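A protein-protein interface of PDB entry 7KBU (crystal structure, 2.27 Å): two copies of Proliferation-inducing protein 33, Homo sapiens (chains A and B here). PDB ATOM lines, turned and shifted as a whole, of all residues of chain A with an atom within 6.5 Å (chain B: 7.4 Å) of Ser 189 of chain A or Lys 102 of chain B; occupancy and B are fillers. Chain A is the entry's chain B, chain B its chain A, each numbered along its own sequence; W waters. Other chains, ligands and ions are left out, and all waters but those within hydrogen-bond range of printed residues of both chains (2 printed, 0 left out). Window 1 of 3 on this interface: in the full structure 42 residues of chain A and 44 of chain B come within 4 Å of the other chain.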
ATOM      1  N   ASP A  74     -31.413  -5.213 -11.262  1.00  0.00           N
ATOM      2  CA  ASP A  74     -29.986  -5.009 -10.997  1.00  0.00           C
ATOM      3  C   ASP A  74     -29.110  -5.826 -11.946  1.00  0.00           C
ATOM      4  O   ASP A  74     -28.377  -5.251 -12.754  1.00  0.00           O
ATOM      5  CB  ASP A  74     -29.659  -5.349  -9.528  1.00  0.00           C
ATOM      6  CG  ASP A  74     -28.378  -4.674  -9.038  1.00  0.00           C
ATOM      7  OD1 ASP A  74     -27.549  -4.254  -9.884  1.00  0.00           O
ATOM      8  OD2 ASP A  74     -28.202  -4.559  -7.800  1.00  0.00           O
ATOM      9  N   TYR A  75     -29.256  -7.151 -11.938  1.00  0.00           N
ATOM     10  CA  TYR A  75     -28.531  -8.011 -12.863  1.00  0.00           C
ATOM     11  C   TYR A  75     -29.286  -9.326 -13.005  1.00  0.00           C
ATOM     12  O   TYR A  75     -30.203  -9.630 -12.231  1.00  0.00           O
ATOM     13  CB  TYR A  75     -27.078  -8.246 -12.410  1.00  0.00           C
ATOM     14  CG  TYR A  75     -26.888  -8.712 -10.974  1.00  0.00           C
ATOM     15  CD1 TYR A  75     -26.918 -10.060 -10.650  1.00  0.00           C
ATOM     16  CD2 TYR A  75     -26.640  -7.799  -9.947  1.00  0.00           C
ATOM     17  CE1 TYR A  75     -26.744 -10.491  -9.334  1.00  0.00           C
ATOM     18  CE2 TYR A  75     -26.460  -8.226  -8.629  1.00  0.00           C
ATOM     19  CZ  TYR A  75     -26.515  -9.573  -8.330  1.00  0.00           C
ATOM     20  OH  TYR A  75     -26.330 -10.005  -7.023  1.00  0.00           O
ATOM     21  N   VAL A  90     -13.582  -2.012 -14.589  1.00  0.00           N
ATOM     22  CA  VAL A  90     -14.546  -1.346 -15.453  1.00  0.00           C
ATOM     23  C   VAL A  90     -13.920  -0.997 -16.802  1.00  0.00           C
ATOM     24  O   VAL A  90     -14.566  -1.125 -17.849  1.00  0.00           O
ATOM     25  CB  VAL A  90     -15.120  -0.081 -14.792  1.00  0.00           C
ATOM     26  CG1 VAL A  90     -16.046   0.615 -15.785  1.00  0.00           C
ATOM     27  CG2 VAL A  90     -15.858  -0.382 -13.486  1.00  0.00           C
ATOM     28  N   GLN A  92     -11.930  -1.539 -19.958  1.00  0.00           N
ATOM     29  CA  GLN A  92     -11.487  -2.701 -20.728  1.00  0.00           C
ATOM     30  C   GLN A  92     -10.228  -2.326 -21.503  1.00  0.00           C
ATOM     31  O   GLN A  92     -10.267  -1.421 -22.340  1.00  0.00           O
ATOM     32  CB  GLN A  92     -12.609  -3.142 -21.673  1.00  0.00           C
ATOM     33  CG  GLN A  92     -13.893  -3.551 -20.942  1.00  0.00           C
ATOM     34  CD  GLN A  92     -13.644  -4.712 -20.012  1.00  0.00           C
ATOM     35  OE1 GLN A  92     -12.878  -5.628 -20.344  1.00  0.00           O
ATOM     36  NE2 GLN A  92     -14.258  -4.676 -18.824  1.00  0.00           N
ATOM     37  N   TRP A 164     -13.954   8.051 -22.913  1.00  0.00           N
ATOM     38  CA  TRP A 164     -14.774   7.361 -23.905  1.00  0.00           C
ATOM     39  C   TRP A 164     -15.912   6.588 -23.235  1.00  0.00           C
ATOM     40  O   TRP A 164     -17.045   6.584 -23.727  1.00  0.00           O
ATOM     41  CB  TRP A 164     -13.898   6.414 -24.736  1.00  0.00           C
ATOM     42  CG  TRP A 164     -14.684   5.476 -25.595  1.00  0.00           C
ATOM     43  CD1 TRP A 164     -15.114   5.710 -26.865  1.00  0.00           C
ATOM     44  CD2 TRP A 164     -15.148   4.158 -25.247  1.00  0.00           C
ATOM     45  NE1 TRP A 164     -15.823   4.626 -27.330  1.00  0.00           N
ATOM     46  CE2 TRP A 164     -15.856   3.660 -26.358  1.00  0.00           C
ATOM     47  CE3 TRP A 164     -15.032   3.353 -24.104  1.00  0.00           C
ATOM     48  CZ2 TRP A 164     -16.441   2.390 -26.370  1.00  0.00           C
ATOM     49  CZ3 TRP A 164     -15.621   2.094 -24.114  1.00  0.00           C
ATOM     50  CH2 TRP A 164     -16.321   1.631 -25.237  1.00  0.00           C
ATOM     51  N   GLN A 165     -15.649   5.971 -22.090  1.00  0.00           N
ATOM     52  CA  GLN A 165     -16.709   5.210 -21.425  1.00  0.00           C
ATOM     53  C   GLN A 165     -17.824   6.127 -20.923  1.00  0.00           C
ATOM     54  O   GLN A 165     -19.007   5.784 -21.021  1.00  0.00           O
ATOM     55  CB  GLN A 165     -16.124   4.374 -20.288  1.00  0.00           C
ATOM     56  CG  GLN A 165     -17.155   3.558 -19.523  1.00  0.00           C
ATOM     57  CD  GLN A 165     -17.701   2.400 -20.332  1.00  0.00           C
ATOM     58  OE1 GLN A 165     -17.223   1.277 -20.212  1.00  0.00           O
ATOM     59  NE2 GLN A 165     -18.708   2.672 -21.162  1.00  0.00           N
ATOM     60  N   ALA A 184     -27.088   1.799 -15.210  1.00  0.00           N
ATOM     61  CA  ALA A 184     -27.659   0.491 -14.829  1.00  0.00           C
ATOM     62  C   ALA A 184     -27.315  -0.612 -15.828  1.00  0.00           C
ATOM     63  O   ALA A 184     -27.104  -1.698 -15.359  1.00  0.00           O
ATOM     64  CB  ALA A 184     -29.136   0.596 -14.632  1.00  0.00           C
ATOM     65  N   PRO A 185     -27.357  -0.426 -17.167  1.00  0.00           N
ATOM     66  CA  PRO A 185     -26.929  -1.491 -18.074  1.00  0.00           C
ATOM     67  C   PRO A 185     -25.433  -1.844 -17.931  1.00  0.00           C
ATOM     68  O   PRO A 185     -25.174  -2.982 -18.064  1.00  0.00           O
ATOM     69  CB  PRO A 185     -27.402  -0.983 -19.445  1.00  0.00           C
ATOM     70  CG  PRO A 185     -27.487   0.494 -19.310  1.00  0.00           C
ATOM     71  CD  PRO A 185     -27.980   0.687 -17.904  1.00  0.00           C
ATOM     72  N   LEU A 186     -24.531  -0.890 -17.658  1.00  0.00           N
ATOM     73  CA  LEU A 186     -23.086  -1.149 -17.433  1.00  0.00           C
ATOM     74  C   LEU A 186     -22.953  -2.023 -16.182  1.00  0.00           C
ATOM     75  O   LEU A 186     -22.150  -2.899 -16.182  1.00  0.00           O
ATOM     76  CB  LEU A 186     -22.274   0.144 -17.274  1.00  0.00           C
ATOM     77  CG  LEU A 186     -20.785  -0.019 -16.941  1.00  0.00           C
ATOM     78  CD1 LEU A 186     -20.047  -0.824 -18.008  1.00  0.00           C
ATOM     79  CD2 LEU A 186     -20.103   1.327 -16.725  1.00  0.00           C
ATOM     80  N   ARG A 187     -23.657  -1.704 -15.117  1.00  0.00           N
ATOM     81  CA  ARG A 187     -23.636  -2.504 -13.894  1.00  0.00           C
ATOM     82  C   ARG A 187     -24.020  -3.956 -14.153  1.00  0.00           C
ATOM     83  O   ARG A 187     -23.335  -4.880 -13.702  1.00  0.00           O
ATOM     84  CB  ARG A 187     -24.592  -1.884 -12.878  1.00  0.00           C
ATOM     85  CG  ARG A 187     -24.679  -2.575 -11.573  1.00  0.00           C
ATOM     86  CD  ARG A 187     -25.463  -1.715 -10.558  1.00  0.00           C
ATOM     87  NE  ARG A 187     -26.807  -1.444 -11.061  1.00  0.00           N
ATOM     88  CZ  ARG A 187     -27.758  -0.821 -10.379  1.00  0.00           C
ATOM     89  NH1 ARG A 187     -27.534  -0.339  -9.164  1.00  0.00           N
ATOM     90  NH2 ARG A 187     -28.970  -0.699 -10.918  1.00  0.00           N
ATOM     91  N   ALA A 188     -25.127  -4.173 -14.861  1.00  0.00           N
ATOM     92  CA  ALA A 188     -25.580  -5.534 -15.123  1.00  0.00           C
ATOM     93  C   ALA A 188     -24.606  -6.301 -16.020  1.00  0.00           C
ATOM     94  O   ALA A 188     -24.481  -7.530 -15.908  1.00  0.00           O
ATOM     95  CB  ALA A 188     -26.971  -5.492 -15.750  1.00  0.00           C
ATOM     96  N   SER A 189     -23.921  -5.620 -16.925  1.00  0.00           N
ATOM     97  CA  SER A 189     -23.002  -6.357 -17.793  1.00  0.00           C
ATOM     98  C   SER A 189     -21.723  -6.743 -17.051  1.00  0.00           C
ATOM     99  O   SER A 189     -21.143  -7.806 -17.325  1.00  0.00           O
ATOM    100  CB  SER A 189     -22.696  -5.531 -19.039  1.00  0.00           C
ATOM    101  OG  SER A 189     -21.817  -4.458 -18.745  1.00  0.00           O
ATOM    102  N   LEU A 190     -21.323  -5.947 -16.059  1.00  0.00           N
ATOM    103  CA  LEU A 190     -20.096  -6.216 -15.327  1.00  0.00           C
ATOM    104  C   LEU A 190     -20.228  -7.340 -14.314  1.00  0.00           C
ATOM    105  O   LEU A 190     -19.215  -7.949 -13.961  1.00  0.00           O
ATOM    106  CB  LEU A 190     -19.633  -4.936 -14.639  1.00  0.00           C
ATOM    107  CG  LEU A 190     -19.065  -3.930 -15.647  1.00  0.00           C
ATOM    108  CD1 LEU A 190     -18.844  -2.615 -14.981  1.00  0.00           C
ATOM    109  CD2 LEU A 190     -17.769  -4.465 -16.245  1.00  0.00           C
ATOM    110  N   VAL A 191     -21.431  -7.658 -13.850  1.00  0.00           N
ATOM    111  CA  VAL A 191     -21.571  -8.777 -12.918  1.00  0.00           C
ATOM    112  C   VAL A 191     -21.081 -10.074 -13.564  1.00  0.00           C
ATOM    113  O   VAL A 191     -20.195 -10.743 -13.007  1.00  0.00           O
ATOM    114  CB  VAL A 191     -23.022  -8.900 -12.428  1.00  0.00           C
ATOM    115  CG1 VAL A 191     -23.214 -10.207 -11.631  1.00  0.00           C
ATOM    116  CG2 VAL A 191     -23.356  -7.706 -11.589  1.00  0.00           C
ATOM    117  N   PRO A 192     -21.622 -10.495 -14.712  1.00  0.00           N
ATOM    118  CA  PRO A 192     -21.090 -11.708 -15.354  1.00  0.00           C
ATOM    119  C   PRO A 192     -19.699 -11.552 -15.939  1.00  0.00           C
ATOM    120  O   PRO A 192     -18.945 -12.535 -15.986  1.00  0.00           O
ATOM    121  CB  PRO A 192     -22.120 -12.006 -16.459  1.00  0.00           C
ATOM    122  CG  PRO A 192     -22.833 -10.733 -16.683  1.00  0.00           C
ATOM    123  CD  PRO A 192     -22.828 -10.001 -15.387  1.00  0.00           C
ATOM    124  N   MET A 193     -19.346 -10.372 -16.441  1.00  0.00           N
ATOM    125  CA  MET A 193     -18.050 -10.231 -17.103  1.00  0.00           C
ATOM    126  C   MET A 193     -16.903 -10.042 -16.120  1.00  0.00           C
ATOM    127  O   MET A 193     -15.784 -10.451 -16.419  1.00  0.00           O
ATOM    128  CB  MET A 193     -18.072  -9.078 -18.091  1.00  0.00           C
ATOM    129  CG  MET A 193     -19.000  -9.352 -19.266  1.00  0.00           C
ATOM    130  SD  MET A 193     -18.970  -8.041 -20.504  1.00  0.00           S
ATOM    131  CE  MET A 193     -17.229  -7.963 -20.940  1.00  0.00           C
ATOM    132  N   GLU A 194     -17.144  -9.432 -14.960  1.00  0.00           N
ATOM    133  CA  GLU A 194     -16.068  -9.102 -14.033  1.00  0.00           C
ATOM    134  C   GLU A 194     -16.325  -9.565 -12.613  1.00  0.00           C
ATOM    135  O   GLU A 194     -15.414  -9.476 -11.785  1.00  0.00           O
ATOM    136  CB  GLU A 194     -15.806  -7.587 -14.018  1.00  0.00           C
ATOM    137  CG  GLU A 194     -14.876  -7.164 -15.142  1.00  0.00           C
ATOM    138  CD  GLU A 194     -13.455  -7.757 -14.999  1.00  0.00           C
ATOM    139  OE1 GLU A 194     -13.035  -8.186 -13.869  1.00  0.00           O
ATOM    140  OE2 GLU A 194     -12.759  -7.787 -16.037  1.00  0.00           O
ATOM    141  N   ARG B  96     -12.561  -6.284 -28.914  1.00  0.00           N
ATOM    142  CA  ARG B  96     -13.752  -6.285 -29.756  1.00  0.00           C
ATOM    143  C   ARG B  96     -14.786  -7.274 -29.232  1.00  0.00           C
ATOM    144  O   ARG B  96     -15.989  -6.990 -29.223  1.00  0.00           O
ATOM    145  CB  ARG B  96     -13.390  -6.650 -31.199  1.00  0.00           C
ATOM    146  CG  ARG B  96     -12.627  -5.580 -31.966  1.00  0.00           C
ATOM    147  CD  ARG B  96     -13.498  -4.378 -32.163  1.00  0.00           C
ATOM    148  NE  ARG B  96     -13.046  -3.496 -33.232  1.00  0.00           N
ATOM    149  CZ  ARG B  96     -13.501  -2.258 -33.393  1.00  0.00           C
ATOM    150  NH1 ARG B  96     -14.391  -1.736 -32.557  1.00  0.00           N
ATOM    151  NH2 ARG B  96     -13.065  -1.530 -34.420  1.00  0.00           N
ATOM    152  N   MET B  97     -14.334  -8.459 -28.817  1.00  0.00           N
ATOM    153  CA  MET B  97     -15.268  -9.456 -28.312  1.00  0.00           C
ATOM    154  C   MET B  97     -15.828  -9.043 -26.960  1.00  0.00           C
ATOM    155  O   MET B  97     -16.989  -9.338 -26.657  1.00  0.00           O
ATOM    156  CB  MET B  97     -14.593 -10.826 -28.242  1.00  0.00           C
ATOM    157  CG  MET B  97     -15.542 -11.959 -27.916  1.00  0.00           C
ATOM    158  SD  MET B  97     -16.629 -12.494 -29.265  1.00  0.00           S
ATOM    159  CE  MET B  97     -15.634 -12.240 -30.725  1.00  0.00           C
ATOM    160  N   ARG B  98     -15.036  -8.357 -26.138  1.00  0.00           N
ATOM    161  CA  ARG B  98     -15.560  -7.889 -24.864  1.00  0.00           C
ATOM    162  C   ARG B  98     -16.560  -6.760 -25.062  1.00  0.00           C
ATOM    163  O   ARG B  98     -17.520  -6.660 -24.294  1.00  0.00           O
ATOM    164  CB  ARG B  98     -14.423  -7.446 -23.945  1.00  0.00           C
ATOM    165  CG  ARG B  98     -13.759  -8.617 -23.194  1.00  0.00           C
ATOM    166  CD  ARG B  98     -12.526  -8.179 -22.359  1.00  0.00           C
ATOM    167  NE  ARG B  98     -11.324  -8.198 -23.183  1.00  0.00           N
ATOM    168  CZ  ARG B  98     -10.337  -7.311 -23.116  1.00  0.00           C
ATOM    169  NH1 ARG B  98     -10.340  -6.347 -22.214  1.00  0.00           N
ATOM    170  NH2 ARG B  98      -9.318  -7.402 -23.973  1.00  0.00           N
ATOM    171  N   ASP B  99     -16.365  -5.904 -26.076  1.00  0.00           N
ATOM    172  CA  ASP B  99     -17.377  -4.890 -26.372  1.00  0.00           C
ATOM    173  C   ASP B  99     -18.669  -5.524 -26.859  1.00  0.00           C
ATOM    174  O   ASP B  99     -19.763  -5.053 -26.533  1.00  0.00           O
ATOM    175  CB  ASP B  99     -16.900  -3.918 -27.439  1.00  0.00           C
ATOM    176  CG  ASP B  99     -15.669  -3.167 -27.045  1.00  0.00           C
ATOM    177  OD1 ASP B  99     -15.624  -2.583 -25.937  1.00  0.00           O
ATOM    178  OD2 ASP B  99     -14.779  -3.081 -27.908  1.00  0.00           O
ATOM    179  N   TRP B 100     -18.556  -6.562 -27.687  1.00  0.00           N
ATOM    180  CA  TRP B 100     -19.738  -7.246 -28.188  1.00  0.00           C
ATOM    181  C   TRP B 100     -20.536  -7.859 -27.047  1.00  0.00           C
ATOM    182  O   TRP B 100     -21.765  -7.756 -26.991  1.00  0.00           O
ATOM    183  CB  TRP B 100     -19.316  -8.326 -29.173  1.00  0.00           C
ATOM    184  CG  TRP B 100     -20.453  -9.199 -29.568  1.00  0.00           C
ATOM    185  CD1 TRP B 100     -21.444  -8.904 -30.479  1.00  0.00           C
ATOM    186  CD2 TRP B 100     -20.741 -10.512 -29.074  1.00  0.00           C
ATOM    187  NE1 TRP B 100     -22.322  -9.957 -30.571  1.00  0.00           N
ATOM    188  CE2 TRP B 100     -21.915 -10.956 -29.724  1.00  0.00           C
ATOM    189  CE3 TRP B 100     -20.119 -11.358 -28.150  1.00  0.00           C
ATOM    190  CZ2 TRP B 100     -22.476 -12.208 -29.477  1.00  0.00           C
ATOM    191  CZ3 TRP B 100     -20.679 -12.595 -27.906  1.00  0.00           C
ATOM    192  CH2 TRP B 100     -21.849 -13.010 -28.564  1.00  0.00           C
ATOM    193  N   LEU B 101     -19.841  -8.524 -26.142  1.00  0.00           N
ATOM    194  CA  LEU B 101     -20.486  -9.157 -25.005  1.00  0.00           C
ATOM    195  C   LEU B 101     -21.133  -8.120 -24.099  1.00  0.00           C
ATOM    196  O   LEU B 101     -22.276  -8.295 -23.644  1.00  0.00           O
ATOM    197  CB  LEU B 101     -19.431  -9.967 -24.267  1.00  0.00           C
ATOM    198  CG  LEU B 101     -19.796 -11.044 -23.262  1.00  0.00           C
ATOM    199  CD1 LEU B 101     -20.727 -12.040 -23.857  1.00  0.00           C
ATOM    200  CD2 LEU B 101     -18.494 -11.714 -22.842  1.00  0.00           C
ATOM    201  N   LYS B 102     -20.431  -7.018 -23.856  1.00  0.00           N
ATOM    202  CA  LYS B 102     -20.986  -5.932 -23.058  1.00  0.00           C
ATOM    203  C   LYS B 102     -22.235  -5.352 -23.717  1.00  0.00           C
ATOM    204  O   LYS B 102     -23.232  -5.063 -23.042  1.00  0.00           O
ATOM    205  CB  LYS B 102     -19.916  -4.861 -22.860  1.00  0.00           C
ATOM    206  CG  LYS B 102     -20.352  -3.669 -22.043  1.00  0.00           C
ATOM    207  CD  LYS B 102     -19.168  -3.032 -21.325  1.00  0.00           C
ATOM    208  CE  LYS B 102     -18.407  -2.072 -22.216  1.00  0.00           C
ATOM    209  NZ  LYS B 102     -17.654  -1.074 -21.388  1.00  0.00           N
ATOM    210  N   ASN B 103     -22.208  -5.191 -25.030  1.00  0.00           N
ATOM    211  CA  ASN B 103     -23.341  -4.581 -25.714  1.00  0.00           C
ATOM    212  C   ASN B 103     -24.571  -5.475 -25.719  1.00  0.00           C
ATOM    213  O   ASN B 103     -25.687  -4.975 -25.598  1.00  0.00           O
ATOM    214  CB  ASN B 103     -22.960  -4.217 -27.142  1.00  0.00           C
ATOM    215  CG  ASN B 103     -22.217  -2.903 -27.213  1.00  0.00           C
ATOM    216  OD1 ASN B 103     -21.146  -2.818 -27.822  1.00  0.00           O
ATOM    217  ND2 ASN B 103     -22.778  -1.863 -26.584  1.00  0.00           N
ATOM    218  N   ILE B 104     -24.413  -6.784 -25.902  1.00  0.00           N
ATOM    219  CA  ILE B 104     -25.603  -7.627 -25.837  1.00  0.00           C
ATOM    220  C   ILE B 104     -26.136  -7.672 -24.406  1.00  0.00           C
ATOM    221  O   ILE B 104     -27.352  -7.743 -24.195  1.00  0.00           O
ATOM    222  CB  ILE B 104     -25.368  -9.029 -26.436  1.00  0.00           C
ATOM    223  CG1 ILE B 104     -24.458  -9.873 -25.562  1.00  0.00           C
ATOM    224  CG2 ILE B 104     -24.858  -8.910 -27.901  1.00  0.00           C
ATOM    225  CD1 ILE B 104     -23.799 -11.045 -26.298  1.00  0.00           C
ATOM    226  N   LEU B 105     -25.248  -7.673 -23.398  1.00  0.00           N
ATOM    227  CA  LEU B 105     -25.735  -7.661 -22.018  1.00  0.00           C
ATOM    228  C   LEU B 105     -26.446  -6.350 -21.717  1.00  0.00           C
ATOM    229  O   LEU B 105     -27.516  -6.343 -21.106  1.00  0.00           O
ATOM    230  CB  LEU B 105     -24.602  -7.893 -21.015  1.00  0.00           C
ATOM    231  CG  LEU B 105     -23.963  -9.277 -21.150  1.00  0.00           C
ATOM    232  CD1 LEU B 105     -22.637  -9.369 -20.418  1.00  0.00           C
ATOM    233  CD2 LEU B 105     -24.910 -10.353 -20.664  1.00  0.00           C
ATOM    234  N   MET B 106     -25.881  -5.229 -22.154  1.00  0.00           N
ATOM    235  CA  MET B 106     -26.556  -3.960 -21.932  1.00  0.00           C
ATOM    236  C   MET B 106     -27.888  -3.933 -22.681  1.00  0.00           C
ATOM    237  O   MET B 106     -28.937  -3.617 -22.105  1.00  0.00           O
ATOM    238  CB  MET B 106     -25.657  -2.804 -22.359  1.00  0.00           C
ATOM    239  CG  MET B 106     -24.533  -2.495 -21.369  1.00  0.00           C
ATOM    240  SD  MET B 106     -23.415  -1.217 -21.978  1.00  0.00           S
ATOM    241  CE  MET B 106     -23.745   0.166 -20.927  1.00  0.00           C
ATOM    242  N   GLN B 107     -27.872  -4.327 -23.955  1.00  0.00           N
ATOM    243  CA  GLN B 107     -29.108  -4.363 -24.733  1.00  0.00           C
ATOM    244  C   GLN B 107     -30.134  -5.306 -24.106  1.00  0.00           C
ATOM    245  O   GLN B 107     -31.322  -4.985 -24.037  1.00  0.00           O
ATOM    246  CB  GLN B 107     -28.794  -4.778 -26.173  1.00  0.00           C
ATOM    247  CG  GLN B 107     -30.014  -4.921 -27.072  1.00  0.00           C
ATOM    248  CD  GLN B 107     -29.654  -4.895 -28.559  1.00  0.00           C
ATOM    249  OE1 GLN B 107     -29.120  -5.872 -29.101  1.00  0.00           O
ATOM    250  NE2 GLN B 107     -29.956  -3.775 -29.226  1.00  0.00           N
ATOM    251  N   LEU B 108     -29.686  -6.457 -23.612  1.00  0.00           N
ATOM    252  CA  LEU B 108     -30.587  -7.382 -22.934  1.00  0.00           C
ATOM    253  C   LEU B 108     -31.178  -6.762 -21.667  1.00  0.00           C
ATOM    254  O   LEU B 108     -32.342  -7.012 -21.332  1.00  0.00           O
ATOM    255  CB  LEU B 108     -29.842  -8.681 -22.615  1.00  0.00           C
ATOM    256  CG  LEU B 108     -30.682  -9.838 -22.073  1.00  0.00           C
ATOM    257  CD1 LEU B 108     -31.658 -10.366 -23.130  1.00  0.00           C
ATOM    258  CD2 LEU B 108     -29.777 -10.953 -21.567  1.00  0.00           C
ATOM    259  N   TYR B 109     -30.393  -5.963 -20.943  1.00  0.00           N
ATOM    260  CA  TYR B 109     -30.910  -5.290 -19.755  1.00  0.00           C
ATOM    261  C   TYR B 109     -31.958  -4.246 -20.124  1.00  0.00           C
ATOM    262  O   TYR B 109     -32.998  -4.140 -19.466  1.00  0.00           O
ATOM    263  CB  TYR B 109     -29.770  -4.632 -18.967  1.00  0.00           C
ATOM    264  CG  TYR B 109     -30.251  -3.808 -17.778  1.00  0.00           C
ATOM    265  CD1 TYR B 109     -30.559  -2.456 -17.913  1.00  0.00           C
ATOM    266  CD2 TYR B 109     -30.390  -4.388 -16.519  1.00  0.00           C
ATOM    267  CE1 TYR B 109     -31.010  -1.701 -16.815  1.00  0.00           C
ATOM    268  CE2 TYR B 109     -30.825  -3.648 -15.418  1.00  0.00           C
ATOM    269  CZ  TYR B 109     -31.138  -2.313 -15.571  1.00  0.00           C
ATOM    270  OH  TYR B 109     -31.586  -1.603 -14.482  1.00  0.00           O
ATOM    271  N   LEU B 138     -26.915 -16.509 -18.262  1.00  0.00           N
ATOM    272  CA  LEU B 138     -26.414 -15.685 -17.165  1.00  0.00           C
ATOM    273  C   LEU B 138     -26.866 -16.218 -15.810  1.00  0.00           C
ATOM    274  O   LEU B 138     -26.112 -16.177 -14.834  1.00  0.00           O
ATOM    275  CB  LEU B 138     -26.871 -14.242 -17.353  1.00  0.00           C
ATOM    276  CG  LEU B 138     -26.785 -13.761 -18.803  1.00  0.00           C
ATOM    277  CD1 LEU B 138     -27.057 -12.279 -18.886  1.00  0.00           C
ATOM    278  CD2 LEU B 138     -25.417 -14.100 -19.371  1.00  0.00           C
ATOM    279  N   ILE B 144     -20.107 -16.859 -19.474  1.00  0.00           N
ATOM    280  CA  ILE B 144     -19.191 -16.380 -20.505  1.00  0.00           C
ATOM    281  C   ILE B 144     -18.469 -17.554 -21.174  1.00  0.00           C
ATOM    282  O   ILE B 144     -18.252 -17.551 -22.393  1.00  0.00           O
ATOM    283  CB  ILE B 144     -18.193 -15.366 -19.914  1.00  0.00           C
ATOM    284  CG1 ILE B 144     -18.915 -14.165 -19.274  1.00  0.00           C
ATOM    285  CG2 ILE B 144     -17.212 -14.875 -20.984  1.00  0.00           C
ATOM    286  CD1 ILE B 144     -20.177 -13.732 -19.974  1.00  0.00           C
HETATM  287  O   HOH W   1     -20.000   1.007 -22.842  1.00  0.00           O
HETATM  288  O   HOH W   2     -16.644  -2.089 -19.263  1.00  0.00           O
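The backbone NH (N) of Lys 102 of chain B lies within hydrogen-bond range of the side-chain sulfur (SD) of Met 193 of chain A, at 3.8 Å.
The guanidinium group of Arg 98 of chain B lies within hydrogen-bond range of the side-chain amide oxygen of Gln 92 of chain A (3.2 Å).
The side-chain amide oxygen (OE1) of Gln 165 of chain A is in hydrogen-bond range of the side-chain amino group (NZ) of Lys 102 of chain B, at 2.7 Å.
OD1 of Asp 74 of chain A is in salt-bridge range of NE of Arg 187 of chain A.
The backbone carbonyl oxygen (O) of Leu 186 of chain A lies within hydrogen-bond range of the side-chain hydroxyl (OG) of Ser 189 of chain A (3.0 Å).
Asp 74 of chain A touches Tyr 109 of chain B.
O of Pro 185 of chain A touches CG of Met 106 of chain B, at 3.4 Å.
Tyr 109 of chain B touches Pro 185 of chain A (CD1 to CA, 3.8 Å).
CE of Met 106 of chain B touches N of Leu 186 of chain A, at 3.5 Å.
CD2 of Tyr 109 of chain B touches CB of Ala 188 of chain A, at 3.7 Å.
OG of Ser 189 of chain A touches CG of Lys 102 of chain B (3.7 Å).
CB of Leu 105 of chain B touches CB of Ser 189 of chain A, at 3.6 Å.
Leu 105 of chain B touches Pro 192 of chain A.
CG1 of Ile 144 of chain B touches O of Pro 192 of chain A, at 3.7 Å.
CD1 of Leu 105 of chain B touches CG of Met 193 of chain A, at 3.8 Å.
Ser 189 of chain A touches just these residues of chain B: Lys 102 and Leu 105.
Ala 188 of chain A touches just one residue of chain B: Tyr 109 (3.7 Å).
Printed residues of chain A within 4 Å of Met 106 of chain B: Pro 185 (3.4 Å) and Leu 186 (3.5 Å).
Of the printed residues of chain B, Leu 186 of chain A touches Met 106 (3.5 Å).
Printed residues of chain B within 4 Å of Ala 184 of chain A: Tyr 109.
Met 97 of chain B touches none of the printed residues of chain A.
The nearest residue of chain A that does not touch Lys 102 of chain B is Leu 186 of chain A (4.1 Å).
Hydrophobic or aromatic side chains of chain B within 4 Å of the printed part of chain A: Leu 105, Met 106, Tyr 109 and Ile 144.
Of the 17 printed residues of chain A, 10 touch a printed residue of chain B.
Hydrophobic or aromatic side chains of chain A within 4 Å of the printed part of chain B: Ala 184, Pro 185, Leu 186, Ala 188, Pro 192 and Met 193.
Among the printed residues, no Asp or Glu carboxylate lies within 4 Å of a Lys or Arg side-chain nitrogen of the other chain.
No position is printed for both chains.
Of the 15 pairs that touch across the chains among the printed residues, none has its exchanged pair printed and touching as well.
Water W2 bridges the side-chain amino group (NZ) of Lys 102 of chain B (2.6 Å) and the backbone carbonyl oxygen (O) of Val 90 of chain A (2.7 Å).
Water W1 bridges the side-chain amide nitrogen (NE2) of Gln 165 of chain A and the side-chain amino group (NZ) of Lys 102 of chain B.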
